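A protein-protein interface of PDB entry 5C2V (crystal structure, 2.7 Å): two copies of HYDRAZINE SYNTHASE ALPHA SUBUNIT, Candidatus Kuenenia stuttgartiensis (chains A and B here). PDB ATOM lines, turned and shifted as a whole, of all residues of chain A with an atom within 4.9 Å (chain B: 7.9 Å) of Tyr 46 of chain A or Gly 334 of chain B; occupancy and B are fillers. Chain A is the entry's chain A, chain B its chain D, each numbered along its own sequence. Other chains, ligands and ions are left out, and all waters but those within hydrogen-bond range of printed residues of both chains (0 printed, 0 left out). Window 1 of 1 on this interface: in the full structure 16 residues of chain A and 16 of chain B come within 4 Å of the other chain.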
ATOM      1  N   ASP A  44       3.765 -21.685 -36.304  1.00  0.00           N
ATOM      2  CA  ASP A  44       2.947 -22.634 -35.558  1.00  0.00           C
ATOM      3  C   ASP A  44       2.415 -21.965 -34.293  1.00  0.00           C
ATOM      4  O   ASP A  44       2.841 -22.296 -33.188  1.00  0.00           O
ATOM      5  CB  ASP A  44       3.761 -23.883 -35.208  1.00  0.00           C
ATOM      6  CG  ASP A  44       2.896 -25.038 -34.733  1.00  0.00           C
ATOM      7  OD1 ASP A  44       1.692 -24.828 -34.480  1.00  0.00           O
ATOM      8  OD2 ASP A  44       3.427 -26.161 -34.609  1.00  0.00           O
ATOM      9  N   PRO A  45       1.479 -21.017 -34.455  1.00  0.00           N
ATOM     10  CA  PRO A  45       0.987 -20.224 -33.325  1.00  0.00           C
ATOM     11  C   PRO A  45      -0.048 -20.964 -32.484  1.00  0.00           C
ATOM     12  O   PRO A  45      -1.170 -20.480 -32.339  1.00  0.00           O
ATOM     13  CB  PRO A  45       0.358 -19.012 -34.009  1.00  0.00           C
ATOM     14  CG  PRO A  45      -0.152 -19.560 -35.299  1.00  0.00           C
ATOM     15  CD  PRO A  45       0.822 -20.635 -35.718  1.00  0.00           C
ATOM     16  N   TYR A  46       0.326 -22.111 -31.926  1.00  0.00           N
ATOM     17  CA  TYR A  46      -0.609 -22.906 -31.138  1.00  0.00           C
ATOM     18  C   TYR A  46      -0.904 -22.270 -29.782  1.00  0.00           C
ATOM     19  O   TYR A  46      -1.782 -22.734 -29.056  1.00  0.00           O
ATOM     20  CB  TYR A  46      -0.081 -24.332 -30.947  1.00  0.00           C
ATOM     21  CG  TYR A  46       1.346 -24.425 -30.452  1.00  0.00           C
ATOM     22  CD1 TYR A  46       1.654 -24.231 -29.111  1.00  0.00           C
ATOM     23  CD2 TYR A  46       2.383 -24.728 -31.325  1.00  0.00           C
ATOM     24  CE1 TYR A  46       2.957 -24.321 -28.657  1.00  0.00           C
ATOM     25  CE2 TYR A  46       3.688 -24.821 -30.879  1.00  0.00           C
ATOM     26  CZ  TYR A  46       3.970 -24.618 -29.545  1.00  0.00           C
ATOM     27  OH  TYR A  46       5.267 -24.711 -29.098  1.00  0.00           O
ATOM     28  N   GLN A  47      -0.174 -21.213 -29.440  1.00  0.00           N
ATOM     29  CA  GLN A  47      -0.414 -20.507 -28.188  1.00  0.00           C
ATOM     30  C   GLN A  47      -1.588 -19.540 -28.331  1.00  0.00           C
ATOM     31  O   GLN A  47      -2.141 -19.069 -27.339  1.00  0.00           O
ATOM     32  CB  GLN A  47       0.843 -19.755 -27.734  1.00  0.00           C
ATOM     33  CG  GLN A  47       1.142 -18.474 -28.505  1.00  0.00           C
ATOM     34  CD  GLN A  47       1.736 -18.731 -29.877  1.00  0.00           C
ATOM     35  OE1 GLN A  47       2.174 -19.840 -30.180  1.00  0.00           O
ATOM     36  NE2 GLN A  47       1.755 -17.700 -30.714  1.00  0.00           N
ATOM     37  N   ASN A  48      -1.955 -19.242 -29.575  1.00  0.00           N
ATOM     38  CA  ASN A  48      -3.084 -18.360 -29.867  1.00  0.00           C
ATOM     39  C   ASN A  48      -4.387 -19.103 -30.181  1.00  0.00           C
ATOM     40  O   ASN A  48      -5.388 -18.482 -30.539  1.00  0.00           O
ATOM     41  CB  ASN A  48      -2.730 -17.421 -31.020  1.00  0.00           C
ATOM     42  CG  ASN A  48      -1.765 -16.327 -30.601  1.00  0.00           C
ATOM     43  OD1 ASN A  48      -0.725 -16.125 -31.227  1.00  0.00           O
ATOM     44  ND2 ASN A  48      -2.107 -15.616 -29.532  1.00  0.00           N
ATOM     45  N   TYR A  49      -4.358 -20.429 -30.057  1.00  0.00           N
ATOM     46  CA  TYR A  49      -5.525 -21.288 -30.279  1.00  0.00           C
ATOM     47  C   TYR A  49      -6.733 -20.791 -29.480  1.00  0.00           C
ATOM     48  O   TYR A  49      -6.570 -20.317 -28.357  1.00  0.00           O
ATOM     49  CB  TYR A  49      -5.185 -22.726 -29.874  1.00  0.00           C
ATOM     50  CG  TYR A  49      -5.777 -23.811 -30.744  1.00  0.00           C
ATOM     51  CD1 TYR A  49      -5.239 -24.097 -31.991  1.00  0.00           C
ATOM     52  CD2 TYR A  49      -6.852 -24.572 -30.304  1.00  0.00           C
ATOM     53  CE1 TYR A  49      -5.767 -25.097 -32.785  1.00  0.00           C
ATOM     54  CE2 TYR A  49      -7.388 -25.575 -31.090  1.00  0.00           C
ATOM     55  CZ  TYR A  49      -6.842 -25.832 -32.330  1.00  0.00           C
ATOM     56  OH  TYR A  49      -7.370 -26.829 -33.117  1.00  0.00           O
ATOM     57  N   TYR A  52      -5.850 -19.788 -34.985  1.00  0.00           N
ATOM     58  CA  TYR A  52      -4.673 -20.494 -35.441  1.00  0.00           C
ATOM     59  C   TYR A  52      -4.593 -20.330 -36.941  1.00  0.00           C
ATOM     60  O   TYR A  52      -5.398 -20.896 -37.686  1.00  0.00           O
ATOM     61  CB  TYR A  52      -4.746 -21.972 -35.035  1.00  0.00           C
ATOM     62  CG  TYR A  52      -3.528 -22.813 -35.354  1.00  0.00           C
ATOM     63  CD1 TYR A  52      -2.383 -22.734 -34.573  1.00  0.00           C
ATOM     64  CD2 TYR A  52      -3.538 -23.714 -36.412  1.00  0.00           C
ATOM     65  CE1 TYR A  52      -1.271 -23.508 -34.851  1.00  0.00           C
ATOM     66  CE2 TYR A  52      -2.432 -24.495 -36.696  1.00  0.00           C
ATOM     67  CZ  TYR A  52      -1.301 -24.387 -35.914  1.00  0.00           C
ATOM     68  OH  TYR A  52      -0.198 -25.161 -36.197  1.00  0.00           O
ATOM     69  N   ASN A 307      -5.145 -21.538 -23.865  1.00  0.00           N
ATOM     70  CA  ASN A 307      -5.020 -21.120 -25.258  1.00  0.00           C
ATOM     71  C   ASN A 307      -4.063 -21.979 -26.086  1.00  0.00           C
ATOM     72  O   ASN A 307      -3.810 -21.677 -27.250  1.00  0.00           O
ATOM     73  CB  ASN A 307      -4.590 -19.653 -25.328  1.00  0.00           C
ATOM     74  CG  ASN A 307      -3.628 -19.272 -24.221  1.00  0.00           C
ATOM     75  OD1 ASN A 307      -3.295 -20.089 -23.362  1.00  0.00           O
ATOM     76  ND2 ASN A 307      -3.176 -18.024 -24.235  1.00  0.00           N
ATOM     77  N   TRP A 308      -3.523 -23.039 -25.491  1.00  0.00           N
ATOM     78  CA  TRP A 308      -2.582 -23.904 -26.203  1.00  0.00           C
ATOM     79  C   TRP A 308      -3.263 -25.037 -26.971  1.00  0.00           C
ATOM     80  O   TRP A 308      -4.249 -25.612 -26.512  1.00  0.00           O
ATOM     81  CB  TRP A 308      -1.552 -24.487 -25.237  1.00  0.00           C
ATOM     82  CG  TRP A 308      -0.398 -23.572 -24.992  1.00  0.00           C
ATOM     83  CD1 TRP A 308      -0.424 -22.208 -24.978  1.00  0.00           C
ATOM     84  CD2 TRP A 308       0.963 -23.951 -24.757  1.00  0.00           C
ATOM     85  NE1 TRP A 308       0.834 -21.714 -24.732  1.00  0.00           N
ATOM     86  CE2 TRP A 308       1.703 -22.763 -24.594  1.00  0.00           C
ATOM     87  CE3 TRP A 308       1.625 -25.178 -24.661  1.00  0.00           C
ATOM     88  CZ2 TRP A 308       3.073 -22.768 -24.341  1.00  0.00           C
ATOM     89  CZ3 TRP A 308       2.985 -25.180 -24.410  1.00  0.00           C
ATOM     90  CH2 TRP A 308       3.694 -23.982 -24.253  1.00  0.00           C
ATOM     91  N   GLY A 309      -2.718 -25.348 -28.145  1.00  0.00           N
ATOM     92  CA  GLY A 309      -3.245 -26.407 -28.988  1.00  0.00           C
ATOM     93  C   GLY A 309      -2.426 -27.682 -28.909  1.00  0.00           C
ATOM     94  O   GLY A 309      -2.782 -28.699 -29.504  1.00  0.00           O
ATOM     95  N   VAL A 310      -1.316 -27.621 -28.180  1.00  0.00           N
ATOM     96  CA  VAL A 310      -0.489 -28.796 -27.938  1.00  0.00           C
ATOM     97  C   VAL A 310      -0.510 -29.119 -26.450  1.00  0.00           C
ATOM     98  O   VAL A 310      -0.759 -28.243 -25.622  1.00  0.00           O
ATOM     99  CB  VAL A 310       0.962 -28.593 -28.415  1.00  0.00           C
ATOM    100  CG1 VAL A 310       0.982 -28.178 -29.877  1.00  0.00           C
ATOM    101  CG2 VAL A 310       1.672 -27.558 -27.559  1.00  0.00           C
ATOM    102  N   ARG A 338      -0.525 -33.747 -30.127  1.00  0.00           N
ATOM    103  CA  ARG A 338      -1.554 -32.921 -30.745  1.00  0.00           C
ATOM    104  C   ARG A 338      -2.270 -33.659 -31.876  1.00  0.00           C
ATOM    105  O   ARG A 338      -1.745 -34.626 -32.437  1.00  0.00           O
ATOM    106  CB  ARG A 338      -0.944 -31.616 -31.268  1.00  0.00           C
ATOM    107  CG  ARG A 338       0.118 -31.824 -32.330  1.00  0.00           C
ATOM    108  CD  ARG A 338       0.929 -30.566 -32.597  1.00  0.00           C
ATOM    109  NE  ARG A 338       0.133 -29.482 -33.160  1.00  0.00           N
ATOM    110  CZ  ARG A 338       0.640 -28.319 -33.560  1.00  0.00           C
ATOM    111  NH1 ARG A 338       1.943 -28.096 -33.461  1.00  0.00           N
ATOM    112  NH2 ARG A 338      -0.153 -27.382 -34.061  1.00  0.00           N
ATOM    113  N   GLN B 312       7.567 -22.045 -18.247  1.00  0.00           N
ATOM    114  CA  GLN B 312       7.686 -20.602 -18.422  1.00  0.00           C
ATOM    115  C   GLN B 312       8.550 -19.982 -17.327  1.00  0.00           C
ATOM    116  O   GLN B 312       9.081 -20.687 -16.467  1.00  0.00           O
ATOM    117  CB  GLN B 312       6.303 -19.949 -18.435  1.00  0.00           C
ATOM    118  CG  GLN B 312       5.384 -20.477 -19.523  1.00  0.00           C
ATOM    119  CD  GLN B 312       5.953 -20.279 -20.915  1.00  0.00           C
ATOM    120  OE1 GLN B 312       6.700 -19.333 -21.164  1.00  0.00           O
ATOM    121  NE2 GLN B 312       5.602 -21.175 -21.829  1.00  0.00           N
ATOM    122  N   THR B 330       7.265 -14.562 -19.309  1.00  0.00           N
ATOM    123  CA  THR B 330       7.271 -15.191 -20.634  1.00  0.00           C
ATOM    124  C   THR B 330       5.907 -15.745 -21.040  1.00  0.00           C
ATOM    125  O   THR B 330       4.896 -15.483 -20.387  1.00  0.00           O
ATOM    126  CB  THR B 330       8.289 -16.355 -20.707  1.00  0.00           C
ATOM    127  OG1 THR B 330       7.979 -17.328 -19.702  1.00  0.00           O
ATOM    128  CG2 THR B 330       9.716 -15.860 -20.512  1.00  0.00           C
ATOM    129  N   GLY B 331       5.892 -16.507 -22.132  1.00  0.00           N
ATOM    130  CA  GLY B 331       4.718 -17.266 -22.524  1.00  0.00           C
ATOM    131  C   GLY B 331       3.961 -16.809 -23.756  1.00  0.00           C
ATOM    132  O   GLY B 331       3.080 -17.518 -24.242  1.00  0.00           O
ATOM    133  N   LYS B 332       4.298 -15.635 -24.275  1.00  0.00           N
ATOM    134  CA  LYS B 332       3.561 -15.085 -25.406  1.00  0.00           C
ATOM    135  C   LYS B 332       4.096 -15.568 -26.756  1.00  0.00           C
ATOM    136  O   LYS B 332       3.476 -15.329 -27.793  1.00  0.00           O
ATOM    137  CB  LYS B 332       3.573 -13.557 -25.340  1.00  0.00           C
ATOM    138  CG  LYS B 332       2.454 -12.991 -24.477  1.00  0.00           C
ATOM    139  CD  LYS B 332       2.854 -11.691 -23.803  1.00  0.00           C
ATOM    140  CE  LYS B 332       2.325 -11.634 -22.377  1.00  0.00           C
ATOM    141  NZ  LYS B 332       3.396 -11.342 -21.387  1.00  0.00           N
ATOM    142  N   ASP B 333       5.252 -16.229 -26.745  1.00  0.00           N
ATOM    143  CA  ASP B 333       5.782 -16.847 -27.960  1.00  0.00           C
ATOM    144  C   ASP B 333       5.489 -18.346 -28.055  1.00  0.00           C
ATOM    145  O   ASP B 333       5.770 -18.974 -29.076  1.00  0.00           O
ATOM    146  CB  ASP B 333       7.293 -16.617 -28.051  1.00  0.00           C
ATOM    147  CG  ASP B 333       8.023 -17.003 -26.778  1.00  0.00           C
ATOM    148  OD1 ASP B 333       7.899 -18.167 -26.339  1.00  0.00           O
ATOM    149  OD2 ASP B 333       8.727 -16.140 -26.214  1.00  0.00           O
ATOM    150  N   GLY B 334       4.916 -18.915 -26.999  1.00  0.00           N
ATOM    151  CA  GLY B 334       4.625 -20.339 -26.965  1.00  0.00           C
ATOM    152  C   GLY B 334       5.836 -21.242 -26.785  1.00  0.00           C
ATOM    153  O   GLY B 334       5.713 -22.466 -26.825  1.00  0.00           O
ATOM    154  N   GLY B 335       7.007 -20.644 -26.581  1.00  0.00           N
ATOM    155  CA  GLY B 335       8.233 -21.408 -26.414  1.00  0.00           C
ATOM    156  C   GLY B 335       8.437 -21.909 -24.996  1.00  0.00           C
ATOM    157  O   GLY B 335       7.716 -21.514 -24.080  1.00  0.00           O
ATOM    158  N   LEU B 336       9.423 -22.784 -24.815  1.00  0.00           N
ATOM    159  CA  LEU B 336       9.730 -23.334 -23.497  1.00  0.00           C
ATOM    160  C   LEU B 336      11.048 -22.795 -22.945  1.00  0.00           C
ATOM    161  O   LEU B 336      12.067 -22.770 -23.641  1.00  0.00           O
ATOM    162  CB  LEU B 336       9.775 -24.864 -23.552  1.00  0.00           C
ATOM    163  CG  LEU B 336       8.447 -25.579 -23.807  1.00  0.00           C
ATOM    164  CD1 LEU B 336       8.633 -27.089 -23.770  1.00  0.00           C
ATOM    165  CD2 LEU B 336       7.396 -25.141 -22.798  1.00  0.00           C
ATOM    166  N   TYR B 337      11.015 -22.370 -21.685  1.00  0.00           N
ATOM    167  CA  TYR B 337      12.182 -21.795 -21.024  1.00  0.00           C
ATOM    168  C   TYR B 337      12.693 -22.687 -19.898  1.00  0.00           C
ATOM    169  O   TYR B 337      11.921 -23.395 -19.250  1.00  0.00           O
ATOM    170  CB  TYR B 337      11.853 -20.409 -20.465  1.00  0.00           C
ATOM    171  CG  TYR B 337      11.626 -19.344 -21.513  1.00  0.00           C
ATOM    172  CD1 TYR B 337      10.423 -19.263 -22.203  1.00  0.00           C
ATOM    173  CD2 TYR B 337      12.611 -18.409 -21.803  1.00  0.00           C
ATOM    174  CE1 TYR B 337      10.212 -18.286 -23.158  1.00  0.00           C
ATOM    175  CE2 TYR B 337      12.409 -17.430 -22.756  1.00  0.00           C
ATOM    176  CZ  TYR B 337      11.207 -17.372 -23.430  1.00  0.00           C
ATOM    177  OH  TYR B 337      11.001 -16.399 -24.380  1.00  0.00           O
ATOM    178  N   TYR B 352      16.389 -21.634 -24.022  1.00  0.00           N
ATOM    179  CA  TYR B 352      15.121 -21.405 -24.692  1.00  0.00           C
ATOM    180  C   TYR B 352      14.951 -22.305 -25.904  1.00  0.00           C
ATOM    181  O   TYR B 352      15.856 -22.431 -26.733  1.00  0.00           O
ATOM    182  CB  TYR B 352      15.021 -19.933 -25.098  1.00  0.00           C
ATOM    183  CG  TYR B 352      13.858 -19.583 -25.999  1.00  0.00           C
ATOM    184  CD1 TYR B 352      12.558 -19.573 -25.516  1.00  0.00           C
ATOM    185  CD2 TYR B 352      14.067 -19.232 -27.326  1.00  0.00           C
ATOM    186  CE1 TYR B 352      11.495 -19.240 -26.334  1.00  0.00           C
ATOM    187  CE2 TYR B 352      13.012 -18.896 -28.151  1.00  0.00           C
ATOM    188  CZ  TYR B 352      11.728 -18.902 -27.649  1.00  0.00           C
ATOM    189  OH  TYR B 352      10.673 -18.570 -28.467  1.00  0.00           O
ATOM    190  N   ALA B 353      13.797 -22.956 -25.986  1.00  0.00           N
ATOM    191  CA  ALA B 353      13.418 -23.650 -27.204  1.00  0.00           C
ATOM    192  C   ALA B 353      12.125 -23.049 -27.730  1.00  0.00           C
ATOM    193  O   ALA B 353      11.055 -23.262 -27.159  1.00  0.00           O
ATOM    194  CB  ALA B 353      13.256 -25.135 -26.947  1.00  0.00           C
ATOM    195  N   GLU B 354      12.232 -22.293 -28.818  1.00  0.00           N
ATOM    196  CA  GLU B 354      11.066 -21.712 -29.466  1.00  0.00           C
ATOM    197  C   GLU B 354      10.118 -22.800 -29.925  1.00  0.00           C
ATOM    198  O   GLU B 354       9.056 -23.028 -29.346  1.00  0.00           O
ATOM    199  CB  GLU B 354      11.497 -20.854 -30.658  1.00  0.00           C
ATOM    200  CG  GLU B 354      10.378 -20.077 -31.328  1.00  0.00           C
ATOM    201  CD  GLU B 354      10.863 -19.304 -32.540  1.00  0.00           C
ATOM    202  OE1 GLU B 354      12.024 -19.510 -32.949  1.00  0.00           O
ATOM    203  OE2 GLU B 354      10.087 -18.487 -33.079  1.00  0.00           O
ATOM    204  N   ARG B 355      10.537 -23.470 -30.987  1.00  0.00           N
ATOM    205  CA  ARG B 355       9.834 -24.617 -31.524  1.00  0.00           C
ATOM    206  C   ARG B 355      10.437 -25.937 -31.075  1.00  0.00           C
ATOM    207  O   ARG B 355      10.209 -26.948 -31.712  1.00  0.00           O
ATOM    208  CB  ARG B 355       9.726 -24.528 -33.042  1.00  0.00           C
ATOM    209  CG  ARG B 355       8.490 -23.725 -33.430  1.00  0.00           C
ATOM    210  CD  ARG B 355       7.318 -24.100 -32.513  1.00  0.00           C
ATOM    211  NE  ARG B 355       6.238 -23.115 -32.504  1.00  0.00           N
ATOM    212  CZ  ARG B 355       5.957 -22.333 -31.464  1.00  0.00           C
ATOM    213  NH1 ARG B 355       6.680 -22.416 -30.356  1.00  0.00           N
ATOM    214  NH2 ARG B 355       4.955 -21.467 -31.531  1.00  0.00           N
ATOM    215  N   GLY B 356      11.267 -25.911 -30.036  1.00  0.00           N
ATOM    216  CA  GLY B 356      11.731 -27.145 -29.425  1.00  0.00           C
ATOM    217  C   GLY B 356      13.194 -27.550 -29.457  1.00  0.00           C
ATOM    218  O   GLY B 356      13.560 -28.567 -28.866  1.00  0.00           O
ATOM    219  N   ALA B 369      10.490 -11.838 -23.453  1.00  0.00           N
ATOM    220  CA  ALA B 369      10.822 -13.064 -24.171  1.00  0.00           C
ATOM    221  C   ALA B 369      12.322 -13.165 -24.439  1.00  0.00           C
ATOM    222  O   ALA B 369      13.095 -12.297 -24.033  1.00  0.00           O
ATOM    223  CB  ALA B 369      10.048 -13.138 -25.479  1.00  0.00           C
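No position is printed for both chains.
Of the 9 pairs that touch across the chains among the printed residues, none has its exchanged pair printed and touching as well.
NH1 of Arg 338 of chain A is in salt-bridge range of OD2 of Asp 44 of chain A, 2.7 Å away.
The side-chain amide oxygen (OE1) of Gln 312 of chain B sits at hydrogen-bond distance from the side-chain hydroxyl (OG1) of Thr 330 of chain B, at 2.8 Å.
OD2 of Asp 333 of chain B sits at hydrogen-bond distance from OH of Tyr 337 of chain B (2.9 Å).
The side-chain amide oxygen (OD1) of Asn 48 of chain A sits at hydrogen-bond distance from the side-chain amide nitrogen (NE2) of Gln 47 of chain A, 3.0 Å away.
The backbone NH of Gly 331 of chain B lies within hydrogen-bond range of the side-chain amide oxygen of Gln 312 of chain B (3.1 Å).
The side-chain amide nitrogen of Gln 312 of chain B sits at hydrogen-bond distance from the backbone carbonyl oxygen of Gly 335 of chain B (3.1 Å).
Gln 47 of chain A touches Lys 332 of chain B.
Gln 47 of chain A touches Asp 333 of chain B.
Gly 334 of chain B touches Gln 47 of chain A (CA to CB, 3.9 Å).
Gln 312 of chain B touches Trp 308 of chain A.
Gly 334 of chain B touches Trp 308 of chain A.
Tyr 46 of chain A touches just these residues of chain B: Gly 334 (3.2 Å) and Arg 355 (3.0 Å).
Gly 334 of chain B touches three residues of chain A.
Of the printed residues of chain B, Asp 44 of chain A touches Arg 355 (2.8 Å).
Of the printed residues of chain A, Lys 332 of chain B touches Gln 47 (3.98 Å).
Tyr 337 of chain B touches none of the printed residues of chain A.
The nearest printed residue of chain A that does not touch Gly 334 of chain B is Val 310 of chain A (6.5 Å).
The nearest printed residue of chain A that does not touch Lys 332 of chain B is Asn 48 of chain A (5.5 Å).
Of the 15 printed residues of chain B, 5 touch a printed residue of chain A.
Of the 12 printed residues of chain A, 4 touch a printed residue of chain B.
Printed residues of chain A that touch a printed residue of chain B: Asp 44, Tyr 46, Gln 47 and Trp 308.
Among the printed residues, 9 pairs touch across the chains.
O of Asp 44 of chain A lies within hydrogen-bond range of NH2 of Arg 355 of chain B (2.8 Å).
OH of Tyr 46 of chain A is in hydrogen-bond range of O of Gly 334 of chain B (3.2 Å).
The side-chain amide oxygen of Gln 47 of chain A is in hydrogen-bond range of the guanidinium group of Arg 355 of chain B.
OH of Tyr 46 of chain A lies within hydrogen-bond range of NH1 of Arg 355 of chain B, at 3.0 Å.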
